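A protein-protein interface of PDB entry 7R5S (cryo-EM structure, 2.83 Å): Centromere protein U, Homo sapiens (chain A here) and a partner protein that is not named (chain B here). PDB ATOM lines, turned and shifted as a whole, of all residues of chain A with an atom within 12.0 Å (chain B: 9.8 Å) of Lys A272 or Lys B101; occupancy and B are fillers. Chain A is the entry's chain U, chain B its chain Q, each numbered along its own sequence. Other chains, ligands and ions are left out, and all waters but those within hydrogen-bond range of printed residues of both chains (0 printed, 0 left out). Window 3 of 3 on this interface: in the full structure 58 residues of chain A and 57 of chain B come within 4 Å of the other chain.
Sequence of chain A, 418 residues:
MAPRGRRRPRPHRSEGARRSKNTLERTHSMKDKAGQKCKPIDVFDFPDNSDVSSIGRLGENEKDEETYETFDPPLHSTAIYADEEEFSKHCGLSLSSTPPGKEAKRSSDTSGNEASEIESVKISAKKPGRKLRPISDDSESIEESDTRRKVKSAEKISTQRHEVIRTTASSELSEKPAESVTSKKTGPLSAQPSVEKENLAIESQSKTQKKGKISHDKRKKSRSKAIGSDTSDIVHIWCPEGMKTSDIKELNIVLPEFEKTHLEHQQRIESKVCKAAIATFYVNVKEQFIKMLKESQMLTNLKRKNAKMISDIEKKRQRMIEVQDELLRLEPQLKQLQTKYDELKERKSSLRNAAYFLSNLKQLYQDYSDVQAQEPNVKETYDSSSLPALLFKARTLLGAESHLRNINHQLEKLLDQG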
ATOM      1  N   HIS A 262      33.870  22.547 -12.594  1.00  0.00           N
ATOM      2  CA  HIS A 262      32.600  22.252 -11.943  1.00  0.00           C
ATOM      3  C   HIS A 262      31.583  23.350 -12.235  1.00  0.00           C
ATOM      4  O   HIS A 262      30.539  23.105 -12.852  1.00  0.00           O
ATOM      5  CB  HIS A 262      32.817  22.091 -10.436  1.00  0.00           C
ATOM      6  CG  HIS A 262      31.648  21.499  -9.712  1.00  0.00           C
ATOM      7  ND1 HIS A 262      31.238  20.198  -9.901  1.00  0.00           N
ATOM      8  CD2 HIS A 262      30.811  22.028  -8.790  1.00  0.00           C
ATOM      9  CE1 HIS A 262      30.194  19.951  -9.130  1.00  0.00           C
ATOM     10  NE2 HIS A 262      29.915  21.045  -8.445  1.00  0.00           N
ATOM     11  N   HIS A 265      30.038  23.842 -15.659  1.00  0.00           N
ATOM     12  CA  HIS A 265      28.921  22.991 -16.047  1.00  0.00           C
ATOM     13  C   HIS A 265      27.599  23.451 -15.446  1.00  0.00           C
ATOM     14  O   HIS A 265      26.559  23.376 -16.111  1.00  0.00           O
ATOM     15  CB  HIS A 265      29.189  21.542 -15.628  1.00  0.00           C
ATOM     16  CG  HIS A 265      30.537  21.032 -16.036  1.00  0.00           C
ATOM     17  ND1 HIS A 265      31.259  20.142 -15.272  1.00  0.00           N
ATOM     18  CD2 HIS A 265      31.293  21.286 -17.131  1.00  0.00           C
ATOM     19  CE1 HIS A 265      32.402  19.871 -15.876  1.00  0.00           C
ATOM     20  NE2 HIS A 265      32.447  20.553 -17.006  1.00  0.00           N
ATOM     21  N   GLN A 266      27.629  23.941 -14.203  1.00  0.00           N
ATOM     22  CA  GLN A 266      26.403  24.320 -13.507  1.00  0.00           C
ATOM     23  C   GLN A 266      25.632  25.386 -14.275  1.00  0.00           C
ATOM     24  O   GLN A 266      24.398  25.434 -14.216  1.00  0.00           O
ATOM     25  CB  GLN A 266      26.738  24.816 -12.098  1.00  0.00           C
ATOM     26  CG  GLN A 266      27.765  23.963 -11.363  1.00  0.00           C
ATOM     27  CD  GLN A 266      27.207  22.637 -10.889  1.00  0.00           C
ATOM     28  OE1 GLN A 266      26.004  22.494 -10.687  1.00  0.00           O
ATOM     29  NE2 GLN A 266      28.083  21.653 -10.721  1.00  0.00           N
ATOM     30  N   ARG A 268      25.147  25.596 -17.406  1.00  0.00           N
ATOM     31  CA  ARG A 268      24.492  25.097 -18.612  1.00  0.00           C
ATOM     32  C   ARG A 268      23.361  24.119 -18.317  1.00  0.00           C
ATOM     33  O   ARG A 268      22.242  24.304 -18.805  1.00  0.00           O
ATOM     34  CB  ARG A 268      25.518  24.439 -19.541  1.00  0.00           C
ATOM     35  CG  ARG A 268      26.195  25.413 -20.491  1.00  0.00           C
ATOM     36  CD  ARG A 268      27.273  24.729 -21.310  1.00  0.00           C
ATOM     37  NE  ARG A 268      28.473  24.481 -20.518  1.00  0.00           N
ATOM     38  CZ  ARG A 268      28.783  23.308 -19.979  1.00  0.00           C
ATOM     39  NH1 ARG A 268      27.985  22.264 -20.152  1.00  0.00           N
ATOM     40  NH2 ARG A 268      29.895  23.179 -19.270  1.00  0.00           N
ATOM     41  N   ILE A 269      23.628  23.077 -17.540  1.00  0.00           N
ATOM     42  CA  ILE A 269      22.602  22.096 -17.204  1.00  0.00           C
ATOM     43  C   ILE A 269      21.726  22.664 -16.094  1.00  0.00           C
ATOM     44  O   ILE A 269      22.193  23.434 -15.247  1.00  0.00           O
ATOM     45  CB  ILE A 269      23.249  20.757 -16.802  1.00  0.00           C
ATOM     46  CG1 ILE A 269      22.186  19.707 -16.476  1.00  0.00           C
ATOM     47  CG2 ILE A 269      24.201  20.947 -15.628  1.00  0.00           C
ATOM     48  CD1 ILE A 269      21.342  19.306 -17.668  1.00  0.00           C
ATOM     49  N   GLU A 270      20.439  22.312 -16.112  1.00  0.00           N
ATOM     50  CA  GLU A 270      19.492  22.831 -15.135  1.00  0.00           C
ATOM     51  C   GLU A 270      18.579  21.777 -14.523  1.00  0.00           C
ATOM     52  O   GLU A 270      17.918  22.075 -13.522  1.00  0.00           O
ATOM     53  CB  GLU A 270      18.623  23.930 -15.767  1.00  0.00           C
ATOM     54  CG  GLU A 270      18.267  23.685 -17.227  1.00  0.00           C
ATOM     55  CD  GLU A 270      17.172  22.649 -17.400  1.00  0.00           C
ATOM     56  OE1 GLU A 270      16.316  22.527 -16.500  1.00  0.00           O
ATOM     57  OE2 GLU A 270      17.165  21.962 -18.443  1.00  0.00           O
ATOM     58  N   SER A 271      18.519  20.570 -15.079  1.00  0.00           N
ATOM     59  CA  SER A 271      17.613  19.554 -14.565  1.00  0.00           C
ATOM     60  C   SER A 271      18.101  19.014 -13.224  1.00  0.00           C
ATOM     61  O   SER A 271      19.297  19.015 -12.923  1.00  0.00           O
ATOM     62  CB  SER A 271      17.470  18.415 -15.574  1.00  0.00           C
ATOM     63  OG  SER A 271      17.310  18.921 -16.887  1.00  0.00           O
ATOM     64  N   LYS A 272      17.149  18.548 -12.416  1.00  0.00           N
ATOM     65  CA  LYS A 272      17.418  18.090 -11.057  1.00  0.00           C
ATOM     66  C   LYS A 272      18.335  16.873 -11.012  1.00  0.00           C
ATOM     67  O   LYS A 272      19.433  16.936 -10.447  1.00  0.00           O
ATOM     68  CB  LYS A 272      16.100  17.772 -10.348  1.00  0.00           C
ATOM     69  CG  LYS A 272      15.002  17.297 -11.287  1.00  0.00           C
ATOM     70  CD  LYS A 272      14.518  15.907 -10.912  1.00  0.00           C
ATOM     71  CE  LYS A 272      13.541  15.360 -11.941  1.00  0.00           C
ATOM     72  NZ  LYS A 272      14.144  15.281 -13.300  1.00  0.00           N
ATOM     73  N   VAL A 273      17.888  15.757 -11.594  1.00  0.00           N
ATOM     74  CA  VAL A 273      18.661  14.520 -11.526  1.00  0.00           C
ATOM     75  C   VAL A 273      19.987  14.631 -12.264  1.00  0.00           C
ATOM     76  O   VAL A 273      20.982  14.038 -11.827  1.00  0.00           O
ATOM     77  CB  VAL A 273      17.846  13.340 -12.080  1.00  0.00           C
ATOM     78  CG1 VAL A 273      16.780  12.923 -11.080  1.00  0.00           C
ATOM     79  CG2 VAL A 273      17.211  13.709 -13.413  1.00  0.00           C
ATOM     80  N   CYS A 274      20.035  15.390 -13.361  1.00  0.00           N
ATOM     81  CA  CYS A 274      21.304  15.621 -14.043  1.00  0.00           C
ATOM     82  C   CYS A 274      22.271  16.382 -13.145  1.00  0.00           C
ATOM     83  O   CYS A 274      23.457  16.048 -13.071  1.00  0.00           O
ATOM     84  CB  CYS A 274      21.070  16.373 -15.352  1.00  0.00           C
ATOM     85  SG  CYS A 274      19.657  15.779 -16.303  1.00  0.00           S
ATOM     86  N   LYS A 275      21.777  17.409 -12.448  1.00  0.00           N
ATOM     87  CA  LYS A 275      22.626  18.148 -11.518  1.00  0.00           C
ATOM     88  C   LYS A 275      23.106  17.265 -10.373  1.00  0.00           C
ATOM     89  O   LYS A 275      24.262  17.377  -9.942  1.00  0.00           O
ATOM     90  CB  LYS A 275      21.866  19.355 -10.966  1.00  0.00           C
ATOM     91  CG  LYS A 275      21.909  20.587 -11.848  1.00  0.00           C
ATOM     92  CD  LYS A 275      23.299  21.188 -11.877  1.00  0.00           C
ATOM     93  CE  LYS A 275      23.278  22.582 -12.474  1.00  0.00           C
ATOM     94  NZ  LYS A 275      22.119  23.381 -11.986  1.00  0.00           N
ATOM     95  N   ALA A 276      22.237  16.384  -9.870  1.00  0.00           N
ATOM     96  CA  ALA A 276      22.634  15.470  -8.803  1.00  0.00           C
ATOM     97  C   ALA A 276      23.732  14.522  -9.273  1.00  0.00           C
ATOM     98  O   ALA A 276      24.729  14.310  -8.570  1.00  0.00           O
ATOM     99  CB  ALA A 276      21.419  14.687  -8.304  1.00  0.00           C
ATOM    100  N   ALA A 277      23.558  13.933 -10.459  1.00  0.00           N
ATOM    101  CA  ALA A 277      24.589  13.062 -11.015  1.00  0.00           C
ATOM    102  C   ALA A 277      25.892  13.820 -11.233  1.00  0.00           C
ATOM    103  O   ALA A 277      26.981  13.292 -10.971  1.00  0.00           O
ATOM    104  CB  ALA A 277      24.104  12.440 -12.324  1.00  0.00           C
ATOM    105  N   ILE A 278      25.799  15.065 -11.711  1.00  0.00           N
ATOM    106  CA  ILE A 278      26.985  15.894 -11.908  1.00  0.00           C
ATOM    107  C   ILE A 278      27.739  16.055 -10.596  1.00  0.00           C
ATOM    108  O   ILE A 278      28.940  15.771 -10.508  1.00  0.00           O
ATOM    109  CB  ILE A 278      26.594  17.260 -12.498  1.00  0.00           C
ATOM    110  CG1 ILE A 278      26.288  17.129 -13.990  1.00  0.00           C
ATOM    111  CG2 ILE A 278      27.700  18.283 -12.272  1.00  0.00           C
ATOM    112  CD1 ILE A 278      27.469  16.681 -14.803  1.00  0.00           C
ATOM    113  N   ALA A 279      27.041  16.513  -9.554  1.00  0.00           N
ATOM    114  CA  ALA A 279      27.688  16.727  -8.263  1.00  0.00           C
ATOM    115  C   ALA A 279      28.300  15.435  -7.730  1.00  0.00           C
ATOM    116  O   ALA A 279      29.451  15.420  -7.274  1.00  0.00           O
ATOM    117  CB  ALA A 279      26.686  17.304  -7.263  1.00  0.00           C
ATOM    118  N   THR A 280      27.547  14.334  -7.797  1.00  0.00           N
ATOM    119  CA  THR A 280      28.025  13.077  -7.231  1.00  0.00           C
ATOM    120  C   THR A 280      29.278  12.587  -7.946  1.00  0.00           C
ATOM    121  O   THR A 280      30.304  12.322  -7.308  1.00  0.00           O
ATOM    122  CB  THR A 280      26.924  12.017  -7.286  1.00  0.00           C
ATOM    123  OG1 THR A 280      26.272  12.065  -8.560  1.00  0.00           O
ATOM    124  CG2 THR A 280      25.899  12.254  -6.185  1.00  0.00           C
ATOM    125  N   PHE A 281      29.224  12.461  -9.275  1.00  0.00           N
ATOM    126  CA  PHE A 281      30.382  11.921  -9.978  1.00  0.00           C
ATOM    127  C   PHE A 281      31.554  12.895  -9.949  1.00  0.00           C
ATOM    128  O   PHE A 281      32.713  12.463  -9.979  1.00  0.00           O
ATOM    129  CB  PHE A 281      30.010  11.538 -11.416  1.00  0.00           C
ATOM    130  CG  PHE A 281      30.417  12.550 -12.449  1.00  0.00           C
ATOM    131  CD1 PHE A 281      31.450  12.275 -13.330  1.00  0.00           C
ATOM    132  CD2 PHE A 281      29.748  13.754 -12.568  1.00  0.00           C
ATOM    133  CE1 PHE A 281      31.824  13.195 -14.289  1.00  0.00           C
ATOM    134  CE2 PHE A 281      30.119  14.677 -13.523  1.00  0.00           C
ATOM    135  CZ  PHE A 281      31.157  14.397 -14.386  1.00  0.00           C
ATOM    136  N   ILE B  95      26.779   5.566 -11.478  1.00  0.00           N
ATOM    137  CA  ILE B  95      25.724   6.535 -11.191  1.00  0.00           C
ATOM    138  C   ILE B  95      24.527   6.343 -12.114  1.00  0.00           C
ATOM    139  O   ILE B  95      23.416   6.769 -11.776  1.00  0.00           O
ATOM    140  CB  ILE B  95      26.240   7.987 -11.272  1.00  0.00           C
ATOM    141  CG1 ILE B  95      26.656   8.350 -12.700  1.00  0.00           C
ATOM    142  CG2 ILE B  95      27.377   8.209 -10.283  1.00  0.00           C
ATOM    143  CD1 ILE B  95      25.705   9.303 -13.395  1.00  0.00           C
ATOM    144  N   LEU B  96      24.717   5.713 -13.276  1.00  0.00           N
ATOM    145  CA  LEU B  96      23.592   5.375 -14.136  1.00  0.00           C
ATOM    146  C   LEU B  96      22.876   4.109 -13.683  1.00  0.00           C
ATOM    147  O   LEU B  96      21.695   3.931 -14.004  1.00  0.00           O
ATOM    148  CB  LEU B  96      24.073   5.216 -15.582  1.00  0.00           C
ATOM    149  CG  LEU B  96      23.032   4.960 -16.674  1.00  0.00           C
ATOM    150  CD1 LEU B  96      22.009   6.084 -16.731  1.00  0.00           C
ATOM    151  CD2 LEU B  96      23.709   4.780 -18.021  1.00  0.00           C
ATOM    152  N   SER B  97      23.561   3.236 -12.939  1.00  0.00           N
ATOM    153  CA  SER B  97      22.921   2.019 -12.446  1.00  0.00           C
ATOM    154  C   SER B  97      21.714   2.338 -11.573  1.00  0.00           C
ATOM    155  O   SER B  97      20.731   1.587 -11.559  1.00  0.00           O
ATOM    156  CB  SER B  97      23.929   1.172 -11.670  1.00  0.00           C
ATOM    157  OG  SER B  97      23.269   0.282 -10.788  1.00  0.00           O
ATOM    158  N   ASN B  98      21.767   3.445 -10.835  1.00  0.00           N
ATOM    159  CA  ASN B  98      20.654   3.858  -9.992  1.00  0.00           C
ATOM    160  C   ASN B  98      19.702   4.822 -10.688  1.00  0.00           C
ATOM    161  O   ASN B  98      18.614   5.079 -10.160  1.00  0.00           O
ATOM    162  CB  ASN B  98      21.176   4.500  -8.703  1.00  0.00           C
ATOM    163  CG  ASN B  98      21.964   3.529  -7.845  1.00  0.00           C
ATOM    164  OD1 ASN B  98      21.396   2.803  -7.029  1.00  0.00           O
ATOM    165  ND2 ASN B  98      23.278   3.512  -8.026  1.00  0.00           N
ATOM    166  N   SER B  99      20.078   5.360 -11.845  1.00  0.00           N
ATOM    167  CA  SER B  99      19.206   6.262 -12.582  1.00  0.00           C
ATOM    168  C   SER B  99      18.090   5.479 -13.262  1.00  0.00           C
ATOM    169  O   SER B  99      18.327   4.433 -13.872  1.00  0.00           O
ATOM    170  CB  SER B  99      20.004   7.049 -13.621  1.00  0.00           C
ATOM    171  OG  SER B  99      21.209   7.546 -13.065  1.00  0.00           O
ATOM    172  N   ILE B 100      16.862   5.993 -13.151  1.00  0.00           N
ATOM    173  CA  ILE B 100      15.679   5.318 -13.662  1.00  0.00           C
ATOM    174  C   ILE B 100      14.999   6.114 -14.768  1.00  0.00           C
ATOM    175  O   ILE B 100      14.593   5.544 -15.788  1.00  0.00           O
ATOM    176  CB  ILE B 100      14.677   5.015 -12.525  1.00  0.00           C
ATOM    177  CG1 ILE B 100      15.395   4.439 -11.301  1.00  0.00           C
ATOM    178  CG2 ILE B 100      13.598   4.061 -13.008  1.00  0.00           C
ATOM    179  CD1 ILE B 100      16.162   3.162 -11.580  1.00  0.00           C
ATOM    180  N   LYS B 101      14.863   7.424 -14.594  1.00  0.00           N
ATOM    181  CA  LYS B 101      14.132   8.271 -15.527  1.00  0.00           C
ATOM    182  C   LYS B 101      15.104   9.083 -16.375  1.00  0.00           C
ATOM    183  O   LYS B 101      16.178   9.471 -15.907  1.00  0.00           O
ATOM    184  CB  LYS B 101      13.161   9.178 -14.755  1.00  0.00           C
ATOM    185  CG  LYS B 101      12.576  10.387 -15.494  1.00  0.00           C
ATOM    186  CD  LYS B 101      13.438  11.637 -15.346  1.00  0.00           C
ATOM    187  CE  LYS B 101      12.822  12.823 -16.071  1.00  0.00           C
ATOM    188  NZ  LYS B 101      13.788  13.947 -16.224  1.00  0.00           N
ATOM    189  N   GLU B 102      14.720   9.329 -17.632  1.00  0.00           N
ATOM    190  CA  GLU B 102      15.512  10.110 -18.584  1.00  0.00           C
ATOM    191  C   GLU B 102      16.887   9.466 -18.801  1.00  0.00           C
ATOM    192  O   GLU B 102      17.932  10.016 -18.462  1.00  0.00           O
ATOM    193  CB  GLU B 102      15.649  11.563 -18.112  1.00  0.00           C
ATOM    194  CG  GLU B 102      15.512  12.594 -19.214  1.00  0.00           C
ATOM    195  CD  GLU B 102      15.935  13.978 -18.768  1.00  0.00           C
ATOM    196  OE1 GLU B 102      16.395  14.113 -17.615  1.00  0.00           O
ATOM    197  OE2 GLU B 102      15.808  14.930 -19.566  1.00  0.00           O
ATOM    198  N   LYS B 103      16.846   8.265 -19.381  1.00  0.00           N
ATOM    199  CA  LYS B 103      18.036   7.421 -19.437  1.00  0.00           C
ATOM    200  C   LYS B 103      19.051   7.927 -20.460  1.00  0.00           C
ATOM    201  O   LYS B 103      20.202   8.217 -20.116  1.00  0.00           O
ATOM    202  CB  LYS B 103      17.630   5.979 -19.750  1.00  0.00           C
ATOM    203  CG  LYS B 103      16.707   5.360 -18.714  1.00  0.00           C
ATOM    204  CD  LYS B 103      17.390   5.263 -17.360  1.00  0.00           C
ATOM    205  CE  LYS B 103      18.106   3.934 -17.197  1.00  0.00           C
ATOM    206  NZ  LYS B 103      17.150   2.796 -17.091  1.00  0.00           N
ATOM    207  N   GLU B 104      18.645   8.037 -21.728  1.00  0.00           N
ATOM    208  CA  GLU B 104      19.628   8.168 -22.801  1.00  0.00           C
ATOM    209  C   GLU B 104      20.224   9.572 -22.890  1.00  0.00           C
ATOM    210  O   GLU B 104      21.417   9.721 -23.183  1.00  0.00           O
ATOM    211  CB  GLU B 104      19.002   7.754 -24.137  1.00  0.00           C
ATOM    212  CG  GLU B 104      17.955   8.706 -24.691  1.00  0.00           C
ATOM    213  CD  GLU B 104      18.485   9.554 -25.831  1.00  0.00           C
ATOM    214  OE1 GLU B 104      19.618   9.296 -26.289  1.00  0.00           O
ATOM    215  OE2 GLU B 104      17.769  10.479 -26.270  1.00  0.00           O
ATOM    216  N   GLU B 105      19.433  10.615 -22.637  1.00  0.00           N
ATOM    217  CA  GLU B 105      19.958  11.962 -22.829  1.00  0.00           C
ATOM    218  C   GLU B 105      20.920  12.373 -21.720  1.00  0.00           C
ATOM    219  O   GLU B 105      21.877  13.110 -21.983  1.00  0.00           O
ATOM    220  CB  GLU B 105      18.818  12.976 -22.945  1.00  0.00           C
ATOM    221  CG  GLU B 105      17.729  12.835 -21.905  1.00  0.00           C
ATOM    222  CD  GLU B 105      16.614  11.908 -22.348  1.00  0.00           C
ATOM    223  OE1 GLU B 105      16.869  10.696 -22.493  1.00  0.00           O
ATOM    224  OE2 GLU B 105      15.482  12.395 -22.553  1.00  0.00           O
ATOM    225  N   ILE B 106      20.708  11.899 -20.489  1.00  0.00           N
ATOM    226  CA  ILE B 106      21.631  12.252 -19.416  1.00  0.00           C
ATOM    227  C   ILE B 106      22.993  11.605 -19.649  1.00  0.00           C
ATOM    228  O   ILE B 106      24.033  12.234 -19.431  1.00  0.00           O
ATOM    229  CB  ILE B 106      21.044  11.889 -18.037  1.00  0.00           C
ATOM    230  CG1 ILE B 106      20.946  10.373 -17.843  1.00  0.00           C
ATOM    231  CG2 ILE B 106      19.689  12.553 -17.847  1.00  0.00           C
ATOM    232  CD1 ILE B 106      21.976   9.809 -16.886  1.00  0.00           C
ATOM    233  N   GLN B 107      23.017  10.359 -20.132  1.00  0.00           N
ATOM    234  CA  GLN B 107      24.300   9.732 -20.430  1.00  0.00           C
ATOM    235  C   GLN B 107      24.926  10.325 -21.686  1.00  0.00           C
ATOM    236  O   GLN B 107      26.157  10.390 -21.789  1.00  0.00           O
ATOM    237  CB  GLN B 107      24.144   8.215 -20.559  1.00  0.00           C
ATOM    238  CG  GLN B 107      23.183   7.756 -21.638  1.00  0.00           C
ATOM    239  CD  GLN B 107      23.201   6.253 -21.836  1.00  0.00           C
ATOM    240  OE1 GLN B 107      22.226   5.663 -22.301  1.00  0.00           O
ATOM    241  NE2 GLN B 107      24.317   5.624 -21.484  1.00  0.00           N
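Glu B102 touches Cys A274.
CG2 of Ile B106 touches SG of Cys A274, at 3.6 Å.
Ala A277 touches Ile B95 (CB to CD1, 3.7 Å).
Of chain B, only Lys B101 comes within 4 Å of Lys A272.
No residue of chain B comes within 4 Å of Val A273.
Cys A274 touches two residues of chain B.
Printed residues of chain B within 4 Å of Ala A277: Ile B95 (3.7 Å).
Ile A278 touches none of the printed residues of chain B.
Printed residues of chain A within 4 Å of Ile B95: Ala A277 (3.7 Å).
Of chain A, only Lys A272 (3.2 Å) comes within 4 Å of Lys B101.
Of chain A, only Cys A274 (3.9 Å) comes within 4 Å of Glu B102.
No residue of chain A comes within 4 Å of Lys B103.
Glu B105 touches none of the printed residues of chain A.
Printed residues of chain A within 4 Å of Ile B106: Cys A274.
The nearest printed residue of chain A that does not touch Ile B95 is Thr A280 (4.4 Å).
OE1 of Glu B102 lies within salt-bridge range of NZ of Lys B101 (3.0 Å).
O of Ala A277 sits at hydrogen-bond distance from OG1 of Thr A280 (2.8 Å).
OG of Ser B99 sits at hydrogen-bond distance from O of Ile B95 (2.7 Å).
The side-chain amino group (NZ) of Lys B101 lies close to the side-chain amino group (NZ) of Lys A272, 3.2 Å away.
Along chain B the printed residues that touch a printed residue of chain A span positions 95 to 106.
Among the printed residues, no Asp or Glu carboxylate lies within 4 Å of a Lys or Arg side-chain nitrogen of the other chain.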
